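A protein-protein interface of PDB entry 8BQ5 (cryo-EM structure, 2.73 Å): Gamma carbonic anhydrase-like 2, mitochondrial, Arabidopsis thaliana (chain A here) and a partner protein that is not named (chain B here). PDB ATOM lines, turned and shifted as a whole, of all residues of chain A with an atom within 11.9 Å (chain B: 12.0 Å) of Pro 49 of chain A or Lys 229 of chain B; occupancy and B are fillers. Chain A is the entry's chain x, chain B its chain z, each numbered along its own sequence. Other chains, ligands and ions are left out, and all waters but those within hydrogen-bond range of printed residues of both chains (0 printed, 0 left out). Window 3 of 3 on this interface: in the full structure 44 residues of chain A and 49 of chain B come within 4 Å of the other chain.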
ATOM      1  N   VAL A  45      -5.158 -22.271  -1.655  1.00  0.00           N
ATOM      2  CA  VAL A  45      -6.432 -22.460  -2.341  1.00  0.00           C
ATOM      3  C   VAL A  45      -6.113 -22.656  -3.819  1.00  0.00           C
ATOM      4  O   VAL A  45      -5.838 -21.695  -4.542  1.00  0.00           O
ATOM      5  CB  VAL A  45      -7.382 -21.283  -2.113  1.00  0.00           C
ATOM      6  CG1 VAL A  45      -8.642 -21.444  -2.948  1.00  0.00           C
ATOM      7  CG2 VAL A  45      -7.737 -21.166  -0.640  1.00  0.00           C
ATOM      8  N   THR A  46      -6.157 -23.908  -4.276  1.00  0.00           N
ATOM      9  CA  THR A  46      -5.801 -24.232  -5.648  1.00  0.00           C
ATOM     10  C   THR A  46      -7.060 -24.551  -6.438  1.00  0.00           C
ATOM     11  O   THR A  46      -7.664 -25.612  -6.217  1.00  0.00           O
ATOM     12  CB  THR A  46      -4.834 -25.413  -5.687  1.00  0.00           C
ATOM     13  OG1 THR A  46      -3.728 -25.151  -4.817  1.00  0.00           O
ATOM     14  CG2 THR A  46      -4.315 -25.625  -7.098  1.00  0.00           C
ATOM     15  N   PRO A  47      -7.489 -23.692  -7.356  1.00  0.00           N
ATOM     16  CA  PRO A  47      -8.734 -23.937  -8.087  1.00  0.00           C
ATOM     17  C   PRO A  47      -8.554 -24.975  -9.188  1.00  0.00           C
ATOM     18  O   PRO A  47      -7.442 -25.336  -9.575  1.00  0.00           O
ATOM     19  CB  PRO A  47      -9.069 -22.565  -8.676  1.00  0.00           C
ATOM     20  CG  PRO A  47      -7.743 -21.917  -8.858  1.00  0.00           C
ATOM     21  CD  PRO A  47      -6.860 -22.418  -7.744  1.00  0.00           C
ATOM     22  N   SER A  48      -9.690 -25.448  -9.697  1.00  0.00           N
ATOM     23  CA  SER A  48      -9.707 -26.364 -10.823  1.00  0.00           C
ATOM     24  C   SER A  48     -10.353 -25.690 -12.021  1.00  0.00           C
ATOM     25  O   SER A  48     -11.420 -25.077 -11.878  1.00  0.00           O
ATOM     26  CB  SER A  48     -10.466 -27.648 -10.477  1.00  0.00           C
ATOM     27  OG  SER A  48     -11.854 -27.507 -10.721  1.00  0.00           O
ATOM     28  N   PRO A  49      -9.736 -25.757 -13.203  1.00  0.00           N
ATOM     29  CA  PRO A  49     -10.332 -25.103 -14.379  1.00  0.00           C
ATOM     30  C   PRO A  49     -11.660 -25.701 -14.802  1.00  0.00           C
ATOM     31  O   PRO A  49     -12.495 -24.977 -15.355  1.00  0.00           O
ATOM     32  CB  PRO A  49      -9.267 -25.293 -15.471  1.00  0.00           C
ATOM     33  CG  PRO A  49      -8.018 -25.721 -14.743  1.00  0.00           C
ATOM     34  CD  PRO A  49      -8.489 -26.460 -13.537  1.00  0.00           C
ATOM     35  N   ASP A  50     -11.886 -26.988 -14.559  1.00  0.00           N
ATOM     36  CA  ASP A  50     -13.068 -27.664 -15.069  1.00  0.00           C
ATOM     37  C   ASP A  50     -14.261 -27.593 -14.123  1.00  0.00           C
ATOM     38  O   ASP A  50     -15.284 -28.228 -14.400  1.00  0.00           O
ATOM     39  CB  ASP A  50     -12.746 -29.129 -15.389  1.00  0.00           C
ATOM     40  CG  ASP A  50     -12.249 -29.897 -14.183  1.00  0.00           C
ATOM     41  OD1 ASP A  50     -11.930 -29.260 -13.158  1.00  0.00           O
ATOM     42  OD2 ASP A  50     -12.183 -31.142 -14.261  1.00  0.00           O
ATOM     43  N   ARG A  51     -14.163 -26.854 -13.020  1.00  0.00           N
ATOM     44  CA  ARG A  51     -15.315 -26.693 -12.143  1.00  0.00           C
ATOM     45  C   ARG A  51     -16.395 -25.877 -12.842  1.00  0.00           C
ATOM     46  O   ARG A  51     -16.121 -24.834 -13.442  1.00  0.00           O
ATOM     47  CB  ARG A  51     -14.914 -26.024 -10.825  1.00  0.00           C
ATOM     48  CG  ARG A  51     -16.082 -25.361 -10.094  1.00  0.00           C
ATOM     49  CD  ARG A  51     -15.650 -24.620  -8.839  1.00  0.00           C
ATOM     50  NE  ARG A  51     -14.973 -25.480  -7.875  1.00  0.00           N
ATOM     51  CZ  ARG A  51     -15.590 -26.275  -7.011  1.00  0.00           C
ATOM     52  NH1 ARG A  51     -16.910 -26.359  -6.969  1.00  0.00           N
ATOM     53  NH2 ARG A  51     -14.866 -27.003  -6.167  1.00  0.00           N
ATOM     54  N   VAL A  52     -17.632 -26.360 -12.755  1.00  0.00           N
ATOM     55  CA  VAL A  52     -18.743 -25.757 -13.482  1.00  0.00           C
ATOM     56  C   VAL A  52     -19.142 -24.453 -12.802  1.00  0.00           C
ATOM     57  O   VAL A  52     -19.411 -24.421 -11.596  1.00  0.00           O
ATOM     58  CB  VAL A  52     -19.929 -26.725 -13.564  1.00  0.00           C
ATOM     59  CG1 VAL A  52     -21.152 -26.035 -14.151  1.00  0.00           C
ATOM     60  CG2 VAL A  52     -19.554 -27.946 -14.383  1.00  0.00           C
ATOM     61  N   LYS A  53     -19.169 -23.349 -13.539  1.00  0.00           N
ATOM     62  CA  LYS A  53     -19.623 -22.046 -12.984  1.00  0.00           C
ATOM     63  C   LYS A  53     -21.109 -21.855 -13.312  1.00  0.00           C
ATOM     64  O   LYS A  53     -21.804 -21.250 -12.490  1.00  0.00           O
ATOM     65  CB  LYS A  53     -18.766 -20.914 -13.557  1.00  0.00           C
ATOM     66  CG  LYS A  53     -17.358 -20.810 -12.990  1.00  0.00           C
ATOM     67  CD  LYS A  53     -16.614 -19.570 -13.440  1.00  0.00           C
ATOM     68  CE  LYS A  53     -17.405 -18.290 -13.272  1.00  0.00           C
ATOM     69  NZ  LYS A  53     -16.730 -17.331 -12.366  1.00  0.00           N
ATOM     70  N   TRP A  54     -21.572 -22.371 -14.455  1.00  0.00           N
ATOM     71  CA  TRP A  54     -22.999 -22.261 -14.864  1.00  0.00           C
ATOM     72  C   TRP A  54     -23.523 -23.616 -15.355  1.00  0.00           C
ATOM     73  O   TRP A  54     -23.054 -24.089 -16.401  1.00  0.00           O
ATOM     74  CB  TRP A  54     -23.186 -21.173 -15.929  1.00  0.00           C
ATOM     75  CG  TRP A  54     -24.548 -21.223 -16.546  1.00  0.00           C
ATOM     76  CD1 TRP A  54     -25.737 -20.969 -15.928  1.00  0.00           C
ATOM     77  CD2 TRP A  54     -24.872 -21.608 -17.893  1.00  0.00           C
ATOM     78  NE1 TRP A  54     -26.773 -21.152 -16.800  1.00  0.00           N
ATOM     79  CE2 TRP A  54     -26.275 -21.546 -18.012  1.00  0.00           C
ATOM     80  CE3 TRP A  54     -24.116 -21.995 -19.005  1.00  0.00           C
ATOM     81  CZ2 TRP A  54     -26.933 -21.843 -19.203  1.00  0.00           C
ATOM     82  CZ3 TRP A  54     -24.768 -22.290 -20.181  1.00  0.00           C
ATOM     83  CH2 TRP A  54     -26.158 -22.216 -20.276  1.00  0.00           C
ATOM     84  N   ASP A  55     -24.470 -24.206 -14.628  1.00  0.00           N
ATOM     85  CA  ASP A  55     -25.058 -25.480 -15.024  1.00  0.00           C
ATOM     86  C   ASP A  55     -26.412 -25.189 -15.663  1.00  0.00           C
ATOM     87  O   ASP A  55     -27.329 -24.706 -14.990  1.00  0.00           O
ATOM     88  CB  ASP A  55     -25.193 -26.404 -13.817  1.00  0.00           C
ATOM     89  CG  ASP A  55     -25.419 -27.848 -14.206  1.00  0.00           C
ATOM     90  OD1 ASP A  55     -26.363 -28.122 -14.976  1.00  0.00           O
ATOM     91  OD2 ASP A  55     -24.651 -28.713 -13.736  1.00  0.00           O
ATOM     92  N   TYR A  56     -26.534 -25.484 -16.959  1.00  0.00           N
ATOM     93  CA  TYR A  56     -27.755 -25.164 -17.692  1.00  0.00           C
ATOM     94  C   TYR A  56     -28.962 -25.938 -17.182  1.00  0.00           C
ATOM     95  O   TYR A  56     -30.099 -25.526 -17.432  1.00  0.00           O
ATOM     96  CB  TYR A  56     -27.555 -25.435 -19.186  1.00  0.00           C
ATOM     97  CG  TYR A  56     -27.598 -26.900 -19.550  1.00  0.00           C
ATOM     98  CD1 TYR A  56     -26.453 -27.676 -19.504  1.00  0.00           C
ATOM     99  CD2 TYR A  56     -28.784 -27.508 -19.945  1.00  0.00           C
ATOM    100  CE1 TYR A  56     -26.487 -29.013 -19.832  1.00  0.00           C
ATOM    101  CE2 TYR A  56     -28.825 -28.845 -20.272  1.00  0.00           C
ATOM    102  CZ  TYR A  56     -27.671 -29.592 -20.214  1.00  0.00           C
ATOM    103  OH  TYR A  56     -27.695 -30.927 -20.539  1.00  0.00           O
ATOM    104  N   ARG A  57     -28.746 -27.056 -16.490  1.00  0.00           N
ATOM    105  CA  ARG A  57     -29.857 -27.839 -15.969  1.00  0.00           C
ATOM    106  C   ARG A  57     -30.414 -27.278 -14.670  1.00  0.00           C
ATOM    107  O   ARG A  57     -31.515 -27.667 -14.267  1.00  0.00           O
ATOM    108  CB  ARG A  57     -29.428 -29.289 -15.750  1.00  0.00           C
ATOM    109  CG  ARG A  57     -28.599 -29.857 -16.880  1.00  0.00           C
ATOM    110  CD  ARG A  57     -27.892 -31.132 -16.475  1.00  0.00           C
ATOM    111  NE  ARG A  57     -26.714 -30.877 -15.657  1.00  0.00           N
ATOM    112  CZ  ARG A  57     -25.892 -31.823 -15.224  1.00  0.00           C
ATOM    113  NH1 ARG A  57     -26.079 -33.094 -15.534  1.00  0.00           N
ATOM    114  NH2 ARG A  57     -24.852 -31.482 -14.468  1.00  0.00           N
ATOM    115  N   VAL A 245     -32.921 -26.601 -24.706  1.00  0.00           N
ATOM    116  CA  VAL A 245     -31.600 -27.221 -24.742  1.00  0.00           C
ATOM    117  C   VAL A 245     -31.261 -27.661 -26.160  1.00  0.00           C
ATOM    118  O   VAL A 245     -30.128 -27.485 -26.628  1.00  0.00           O
ATOM    119  CB  VAL A 245     -31.535 -28.401 -23.754  1.00  0.00           C
ATOM    120  CG1 VAL A 245     -30.142 -29.007 -23.742  1.00  0.00           C
ATOM    121  CG2 VAL A 245     -31.943 -27.957 -22.362  1.00  0.00           C
ATOM    122  N   PHE A 248     -30.409 -24.538 -28.230  1.00  0.00           N
ATOM    123  CA  PHE A 248     -29.154 -23.968 -27.759  1.00  0.00           C
ATOM    124  C   PHE A 248     -27.972 -24.820 -28.207  1.00  0.00           C
ATOM    125  O   PHE A 248     -26.877 -24.300 -28.445  1.00  0.00           O
ATOM    126  CB  PHE A 248     -29.197 -23.836 -26.237  1.00  0.00           C
ATOM    127  CG  PHE A 248     -28.098 -22.993 -25.664  1.00  0.00           C
ATOM    128  CD1 PHE A 248     -27.116 -23.560 -24.875  1.00  0.00           C
ATOM    129  CD2 PHE A 248     -28.054 -21.630 -25.905  1.00  0.00           C
ATOM    130  CE1 PHE A 248     -26.109 -22.786 -24.337  1.00  0.00           C
ATOM    131  CE2 PHE A 248     -27.046 -20.852 -25.371  1.00  0.00           C
ATOM    132  CZ  PHE A 248     -26.071 -21.432 -24.586  1.00  0.00           C
ATOM    133  N   LYS A 249     -28.177 -26.133 -28.321  1.00  0.00           N
ATOM    134  CA  LYS A 249     -27.164 -26.994 -28.924  1.00  0.00           C
ATOM    135  C   LYS A 249     -27.041 -26.731 -30.420  1.00  0.00           C
ATOM    136  O   LYS A 249     -25.931 -26.630 -30.954  1.00  0.00           O
ATOM    137  CB  LYS A 249     -27.510 -28.463 -28.680  1.00  0.00           C
ATOM    138  CG  LYS A 249     -26.975 -29.046 -27.393  1.00  0.00           C
ATOM    139  CD  LYS A 249     -27.060 -30.561 -27.432  1.00  0.00           C
ATOM    140  CE  LYS A 249     -27.983 -31.093 -26.351  1.00  0.00           C
ATOM    141  NZ  LYS A 249     -27.292 -31.281 -25.052  1.00  0.00           N
ATOM    142  N   LEU A 252     -25.131 -23.928 -31.587  1.00  0.00           N
ATOM    143  CA  LEU A 252     -23.722 -24.119 -31.279  1.00  0.00           C
ATOM    144  C   LEU A 252     -23.055 -25.177 -32.146  1.00  0.00           C
ATOM    145  O   LEU A 252     -21.875 -25.474 -31.931  1.00  0.00           O
ATOM    146  CB  LEU A 252     -23.559 -24.502 -29.805  1.00  0.00           C
ATOM    147  CG  LEU A 252     -23.840 -23.409 -28.775  1.00  0.00           C
ATOM    148  CD1 LEU A 252     -23.306 -23.818 -27.414  1.00  0.00           C
ATOM    149  CD2 LEU A 252     -23.251 -22.078 -29.216  1.00  0.00           C
ATOM    150  N   GLU B  37     -34.364 -35.727 -19.651  1.00  0.00           N
ATOM    151  CA  GLU B  37     -33.406 -35.030 -18.804  1.00  0.00           C
ATOM    152  C   GLU B  37     -34.119 -34.256 -17.704  1.00  0.00           C
ATOM    153  O   GLU B  37     -35.071 -33.515 -17.964  1.00  0.00           O
ATOM    154  CB  GLU B  37     -32.551 -34.084 -19.643  1.00  0.00           C
ATOM    155  CG  GLU B  37     -31.475 -33.366 -18.855  1.00  0.00           C
ATOM    156  CD  GLU B  37     -30.302 -32.959 -19.717  1.00  0.00           C
ATOM    157  OE1 GLU B  37     -30.508 -32.709 -20.923  1.00  0.00           O
ATOM    158  OE2 GLU B  37     -29.175 -32.877 -19.186  1.00  0.00           O
ATOM    159  N   LEU B 222     -25.243 -16.402 -21.582  1.00  0.00           N
ATOM    160  CA  LEU B 222     -24.814 -17.681 -20.956  1.00  0.00           C
ATOM    161  C   LEU B 222     -23.568 -18.204 -21.674  1.00  0.00           C
ATOM    162  O   LEU B 222     -23.603 -18.295 -22.913  1.00  0.00           O
ATOM    163  CB  LEU B 222     -25.977 -18.666 -21.062  1.00  0.00           C
ATOM    164  CG  LEU B 222     -27.301 -18.154 -20.503  1.00  0.00           C
ATOM    165  CD1 LEU B 222     -28.459 -19.034 -20.948  1.00  0.00           C
ATOM    166  CD2 LEU B 222     -27.246 -18.052 -18.987  1.00  0.00           C
ATOM    167  N   ASN B 223     -22.518 -18.545 -20.925  1.00  0.00           N
ATOM    168  CA  ASN B 223     -21.244 -19.004 -21.540  1.00  0.00           C
ATOM    169  C   ASN B 223     -21.437 -20.321 -22.291  1.00  0.00           C
ATOM    170  O   ASN B 223     -21.814 -21.315 -21.643  1.00  0.00           O
ATOM    171  CB  ASN B 223     -20.127 -19.155 -20.504  1.00  0.00           C
ATOM    172  CG  ASN B 223     -18.740 -19.154 -21.112  1.00  0.00           C
ATOM    173  OD1 ASN B 223     -18.569 -18.870 -22.297  1.00  0.00           O
ATOM    174  ND2 ASN B 223     -17.738 -19.466 -20.308  1.00  0.00           N
ATOM    175  N   VAL B 224     -21.136 -20.340 -23.595  1.00  0.00           N
ATOM    176  CA  VAL B 224     -21.207 -21.603 -24.315  1.00  0.00           C
ATOM    177  C   VAL B 224     -20.083 -22.550 -23.913  1.00  0.00           C
ATOM    178  O   VAL B 224     -20.197 -23.763 -24.127  1.00  0.00           O
ATOM    179  CB  VAL B 224     -21.195 -21.346 -25.831  1.00  0.00           C
ATOM    180  CG1 VAL B 224     -22.105 -20.175 -26.173  1.00  0.00           C
ATOM    181  CG2 VAL B 224     -19.786 -21.080 -26.311  1.00  0.00           C
ATOM    182  N   ILE B 225     -18.998 -22.029 -23.328  1.00  0.00           N
ATOM    183  CA  ILE B 225     -17.897 -22.887 -22.897  1.00  0.00           C
ATOM    184  C   ILE B 225     -18.336 -23.781 -21.740  1.00  0.00           C
ATOM    185  O   ILE B 225     -18.025 -24.975 -21.712  1.00  0.00           O
ATOM    186  CB  ILE B 225     -16.666 -22.034 -22.524  1.00  0.00           C
ATOM    187  CG1 ILE B 225     -15.899 -21.548 -23.769  1.00  0.00           C
ATOM    188  CG2 ILE B 225     -15.742 -22.800 -21.579  1.00  0.00           C
ATOM    189  CD1 ILE B 225     -15.684 -22.583 -24.868  1.00  0.00           C
ATOM    190  N   GLU B 226     -19.067 -23.221 -20.769  1.00  0.00           N
ATOM    191  CA  GLU B 226     -19.565 -24.030 -19.657  1.00  0.00           C
ATOM    192  C   GLU B 226     -20.615 -25.029 -20.127  1.00  0.00           C
ATOM    193  O   GLU B 226     -20.672 -26.164 -19.635  1.00  0.00           O
ATOM    194  CB  GLU B 226     -20.138 -23.131 -18.562  1.00  0.00           C
ATOM    195  CG  GLU B 226     -19.179 -22.065 -18.077  1.00  0.00           C
ATOM    196  CD  GLU B 226     -18.456 -22.474 -16.813  1.00  0.00           C
ATOM    197  OE1 GLU B 226     -19.009 -23.294 -16.050  1.00  0.00           O
ATOM    198  OE2 GLU B 226     -17.332 -21.981 -16.583  1.00  0.00           O
ATOM    199  N   PHE B 227     -21.464 -24.618 -21.071  1.00  0.00           N
ATOM    200  CA  PHE B 227     -22.410 -25.543 -21.682  1.00  0.00           C
ATOM    201  C   PHE B 227     -21.686 -26.729 -22.304  1.00  0.00           C
ATOM    202  O   PHE B 227     -22.043 -27.889 -22.064  1.00  0.00           O
ATOM    203  CB  PHE B 227     -23.246 -24.803 -22.729  1.00  0.00           C
ATOM    204  CG  PHE B 227     -24.460 -25.559 -23.189  1.00  0.00           C
ATOM    205  CD1 PHE B 227     -25.563 -25.700 -22.365  1.00  0.00           C
ATOM    206  CD2 PHE B 227     -24.499 -26.122 -24.454  1.00  0.00           C
ATOM    207  CE1 PHE B 227     -26.679 -26.393 -22.791  1.00  0.00           C
ATOM    208  CE2 PHE B 227     -25.611 -26.816 -24.886  1.00  0.00           C
ATOM    209  CZ  PHE B 227     -26.703 -26.952 -24.055  1.00  0.00           C
ATOM    210  N   GLU B 228     -20.640 -26.456 -23.088  1.00  0.00           N
ATOM    211  CA  GLU B 228     -19.905 -27.535 -23.738  1.00  0.00           C
ATOM    212  C   GLU B 228     -19.140 -28.385 -22.733  1.00  0.00           C
ATOM    213  O   GLU B 228     -18.977 -29.592 -22.942  1.00  0.00           O
ATOM    214  CB  GLU B 228     -18.952 -26.956 -24.778  1.00  0.00           C
ATOM    215  CG  GLU B 228     -19.356 -27.252 -26.203  1.00  0.00           C
ATOM    216  CD  GLU B 228     -18.637 -26.366 -27.191  1.00  0.00           C
ATOM    217  OE1 GLU B 228     -17.928 -25.440 -26.745  1.00  0.00           O
ATOM    218  OE2 GLU B 228     -18.786 -26.589 -28.410  1.00  0.00           O
ATOM    219  N   LYS B 229     -18.652 -27.775 -21.651  1.00  0.00           N
ATOM    220  CA  LYS B 229     -17.982 -28.538 -20.604  1.00  0.00           C
ATOM    221  C   LYS B 229     -18.942 -29.501 -19.918  1.00  0.00           C
ATOM    222  O   LYS B 229     -18.581 -30.647 -19.626  1.00  0.00           O
ATOM    223  CB  LYS B 229     -17.361 -27.587 -19.582  1.00  0.00           C
ATOM    224  CG  LYS B 229     -16.432 -28.264 -18.585  1.00  0.00           C
ATOM    225  CD  LYS B 229     -16.202 -27.401 -17.350  1.00  0.00           C
ATOM    226  CE  LYS B 229     -16.386 -25.920 -17.644  1.00  0.00           C
ATOM    227  NZ  LYS B 229     -16.094 -25.073 -16.458  1.00  0.00           N
ATOM    228  N   VAL B 230     -20.166 -29.050 -19.636  1.00  0.00           N
ATOM    229  CA  VAL B 230     -21.138 -29.922 -18.986  1.00  0.00           C
ATOM    230  C   VAL B 230     -21.599 -31.019 -19.942  1.00  0.00           C
ATOM    231  O   VAL B 230     -21.788 -32.172 -19.539  1.00  0.00           O
ATOM    232  CB  VAL B 230     -22.320 -29.099 -18.440  1.00  0.00           C
ATOM    233  CG1 VAL B 230     -23.584 -29.931 -18.415  1.00  0.00           C
ATOM    234  CG2 VAL B 230     -22.007 -28.592 -17.047  1.00  0.00           C
ATOM    235  N   LEU B 231     -21.783 -30.680 -21.222  1.00  0.00           N
ATOM    236  CA  LEU B 231     -22.217 -31.675 -22.199  1.00  0.00           C
ATOM    237  C   LEU B 231     -21.189 -32.785 -22.374  1.00  0.00           C
ATOM    238  O   LEU B 231     -21.552 -33.957 -22.529  1.00  0.00           O
ATOM    239  CB  LEU B 231     -22.496 -31.010 -23.546  1.00  0.00           C
ATOM    240  CG  LEU B 231     -23.776 -30.193 -23.685  1.00  0.00           C
ATOM    241  CD1 LEU B 231     -24.155 -30.073 -25.153  1.00  0.00           C
ATOM    242  CD2 LEU B 231     -24.892 -30.834 -22.886  1.00  0.00           C
ATOM    243  N   ARG B 232     -19.904 -32.438 -22.371  1.00  0.00           N
ATOM    244  CA  ARG B 232     -18.850 -33.382 -22.709  1.00  0.00           C
ATOM    245  C   ARG B 232     -18.177 -33.994 -21.484  1.00  0.00           C
ATOM    246  O   ARG B 232     -16.998 -34.356 -21.556  1.00  0.00           O
ATOM    247  CB  ARG B 232     -17.799 -32.707 -23.590  1.00  0.00           C
ATOM    248  CG  ARG B 232     -18.327 -32.193 -24.918  1.00  0.00           C
ATOM    249  CD  ARG B 232     -17.239 -31.444 -25.667  1.00  0.00           C
ATOM    250  NE  ARG B 232     -17.761 -30.682 -26.795  1.00  0.00           N
ATOM    251  CZ  ARG B 232     -17.040 -29.838 -27.522  1.00  0.00           C
ATOM    252  NH1 ARG B 232     -15.755 -29.639 -27.276  1.00  0.00           N
ATOM    253  NH2 ARG B 232     -17.623 -29.178 -28.517  1.00  0.00           N
ATOM    254  N   LYS B 233     -18.889 -34.124 -20.369  1.00  0.00           N
ATOM    255  CA  LYS B 233     -18.292 -34.728 -19.189  1.00  0.00           C
ATOM    256  C   LYS B 233     -18.233 -36.246 -19.328  1.00  0.00           C
ATOM    257  O   LYS B 233     -19.157 -36.884 -19.839  1.00  0.00           O
ATOM    258  CB  LYS B 233     -19.075 -34.352 -17.933  1.00  0.00           C
ATOM    259  CG  LYS B 233     -18.262 -34.479 -16.655  1.00  0.00           C
ATOM    260  CD  LYS B 233     -19.037 -33.986 -15.446  1.00  0.00           C
ATOM    261  CE  LYS B 233     -19.106 -32.467 -15.406  1.00  0.00           C
ATOM    262  NZ  LYS B 233     -17.769 -31.829 -15.534  1.00  0.00           N
ATOM    263  N   LYS B 234     -17.127 -36.822 -18.867  1.00  0.00           N
ATOM    264  CA  LYS B 234     -16.959 -38.271 -18.879  1.00  0.00           C
ATOM    265  C   LYS B 234     -16.357 -38.761 -17.566  1.00  0.00           C
ATOM    266  O   LYS B 234     -16.437 -39.946 -17.239  1.00  0.00           O
ATOM    267  CB  LYS B 234     -16.080 -38.704 -20.052  1.00  0.00           C
ATOM    268  CG  LYS B 234     -16.782 -38.681 -21.398  1.00  0.00           C
ATOM    269  CD  LYS B 234     -15.829 -39.070 -22.513  1.00  0.00           C
ATOM    270  CE  LYS B 234     -16.524 -39.057 -23.863  1.00  0.00           C
ATOM    271  NZ  LYS B 234     -15.600 -39.442 -24.967  1.00  0.00           N
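OD1 of Asp 50 of chain A sits at hydrogen-bond distance from OG of Ser 48 of chain A, at 3.0 Å.
OG of Ser 48 of chain A sits at hydrogen-bond distance from N of Arg 51 of chain A, 3.3 Å away.
The side-chain amide oxygen (OD1) of Asn 223 of chain B sits close to the backbone NH (N) of Ile 225 of chain B, at 3.4 Å.
OD1 of Asp 55 of chain A is in salt-bridge range of NE of Arg 57 of chain A (2.9 Å).
NZ of Lys 229 of chain B lies within salt-bridge range of OE2 of Glu 226 of chain B (3.3 Å).
Hydrophobic or aromatic side chains of chain A within 4 Å of the printed part of chain B: Val 52, Trp 54, Tyr 56, Phe 248 and Leu 252.
Of the 14 printed residues of chain B, 9 touch a printed residue of chain A.
Printed residues of chain B that touch a printed residue of chain A: Glu 37, Leu 222, Asn 223, Val 224, Glu 226, Phe 227, Lys 229, Val 230 and Leu 231.
Hydrophobic or aromatic side chains of chain B that line the printed part of chain A: Leu 222, Val 224, Phe 227, Val 230 and Leu 231.
Among the printed residues, 20 pairs touch across the chains.
Among the printed residues, no Asp or Glu carboxylate lies within 4 Å of a Lys or Arg side-chain nitrogen of the other chain.
Lys 229 of chain B touches Pro 49 of chain A.
CD of Lys 229 of chain B touches O of Asp 50 of chain A (3.2 Å).
Trp 54 of chain A touches Asn 223 of chain B (CZ3 to O, 3.4 Å).
Trp 54 of chain A touches Phe 227 of chain B.
CG of Tyr 56 of chain A touches CE1 of Phe 227 of chain B, at 3.4 Å.
Leu 231 of chain B touches Tyr 56 of chain A.
OE2 of Glu 37 of chain B touches CD of Arg 57 of chain A, 3.5 Å away.
Phe 248 of chain A touches Phe 227 of chain B (CE1 to CG, 3.4 Å).
Lys 249 of chain A touches Phe 227 of chain B.
Leu 252 of chain A touches Val 224 of chain B (CD1 to CB, 3.6 Å).
OE1 of Glu 226 of chain B lies within hydrogen-bond range of N of Trp 54 of chain A.
The side-chain hydroxyl of Tyr 56 of chain A is in hydrogen-bond range of the side-chain carboxylate of Glu 37 of chain B.
The backbone carbonyl oxygen (O) of Arg 51 of chain A sits at hydrogen-bond distance from the side-chain amino group (NZ) of Lys 229 of chain B.
The side-chain carboxylate of Glu 226 of chain B is in hydrogen-bond range of the backbone NH of Lys 53 of chain A (2.5 Å).
No residue of chain B comes within 4 Å of Ser 48 of chain A.
Of the printed residues of chain B, Arg 51 of chain A touches Lys 229.
Printed residues of chain B within 4 Å of Lys 53 of chain A: Glu 226 (2.5 Å).
Val 245 of chain A touches none of the printed residues of chain B.
Printed residues of chain B within 4 Å of Leu 252 of chain A: Val 224 and Phe 227.
Of the printed residues of chain A, Glu 37 of chain B touches Tyr 56 (2.8 Å) and Arg 57 (3.5 Å).
Printed residues of chain A within 4 Å of Val 224 of chain B: Leu 252 (3.6 Å).
Of chain A, only Val 52, Lys 53 and Trp 54 come within 4 Å of Glu 226 of chain B.
Of chain A, only Pro 49, Asp 50 and Arg 51 come within 4 Å of Lys 229 of chain B.
No residue of chain A comes within 4 Å of Arg 232 of chain B.
No residue of chain A comes within 4 Å of Lys 233 of chain B.
The nearest residue of chain B that does not touch Pro 49 of chain A is Glu 226 of chain B (5.8 Å).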
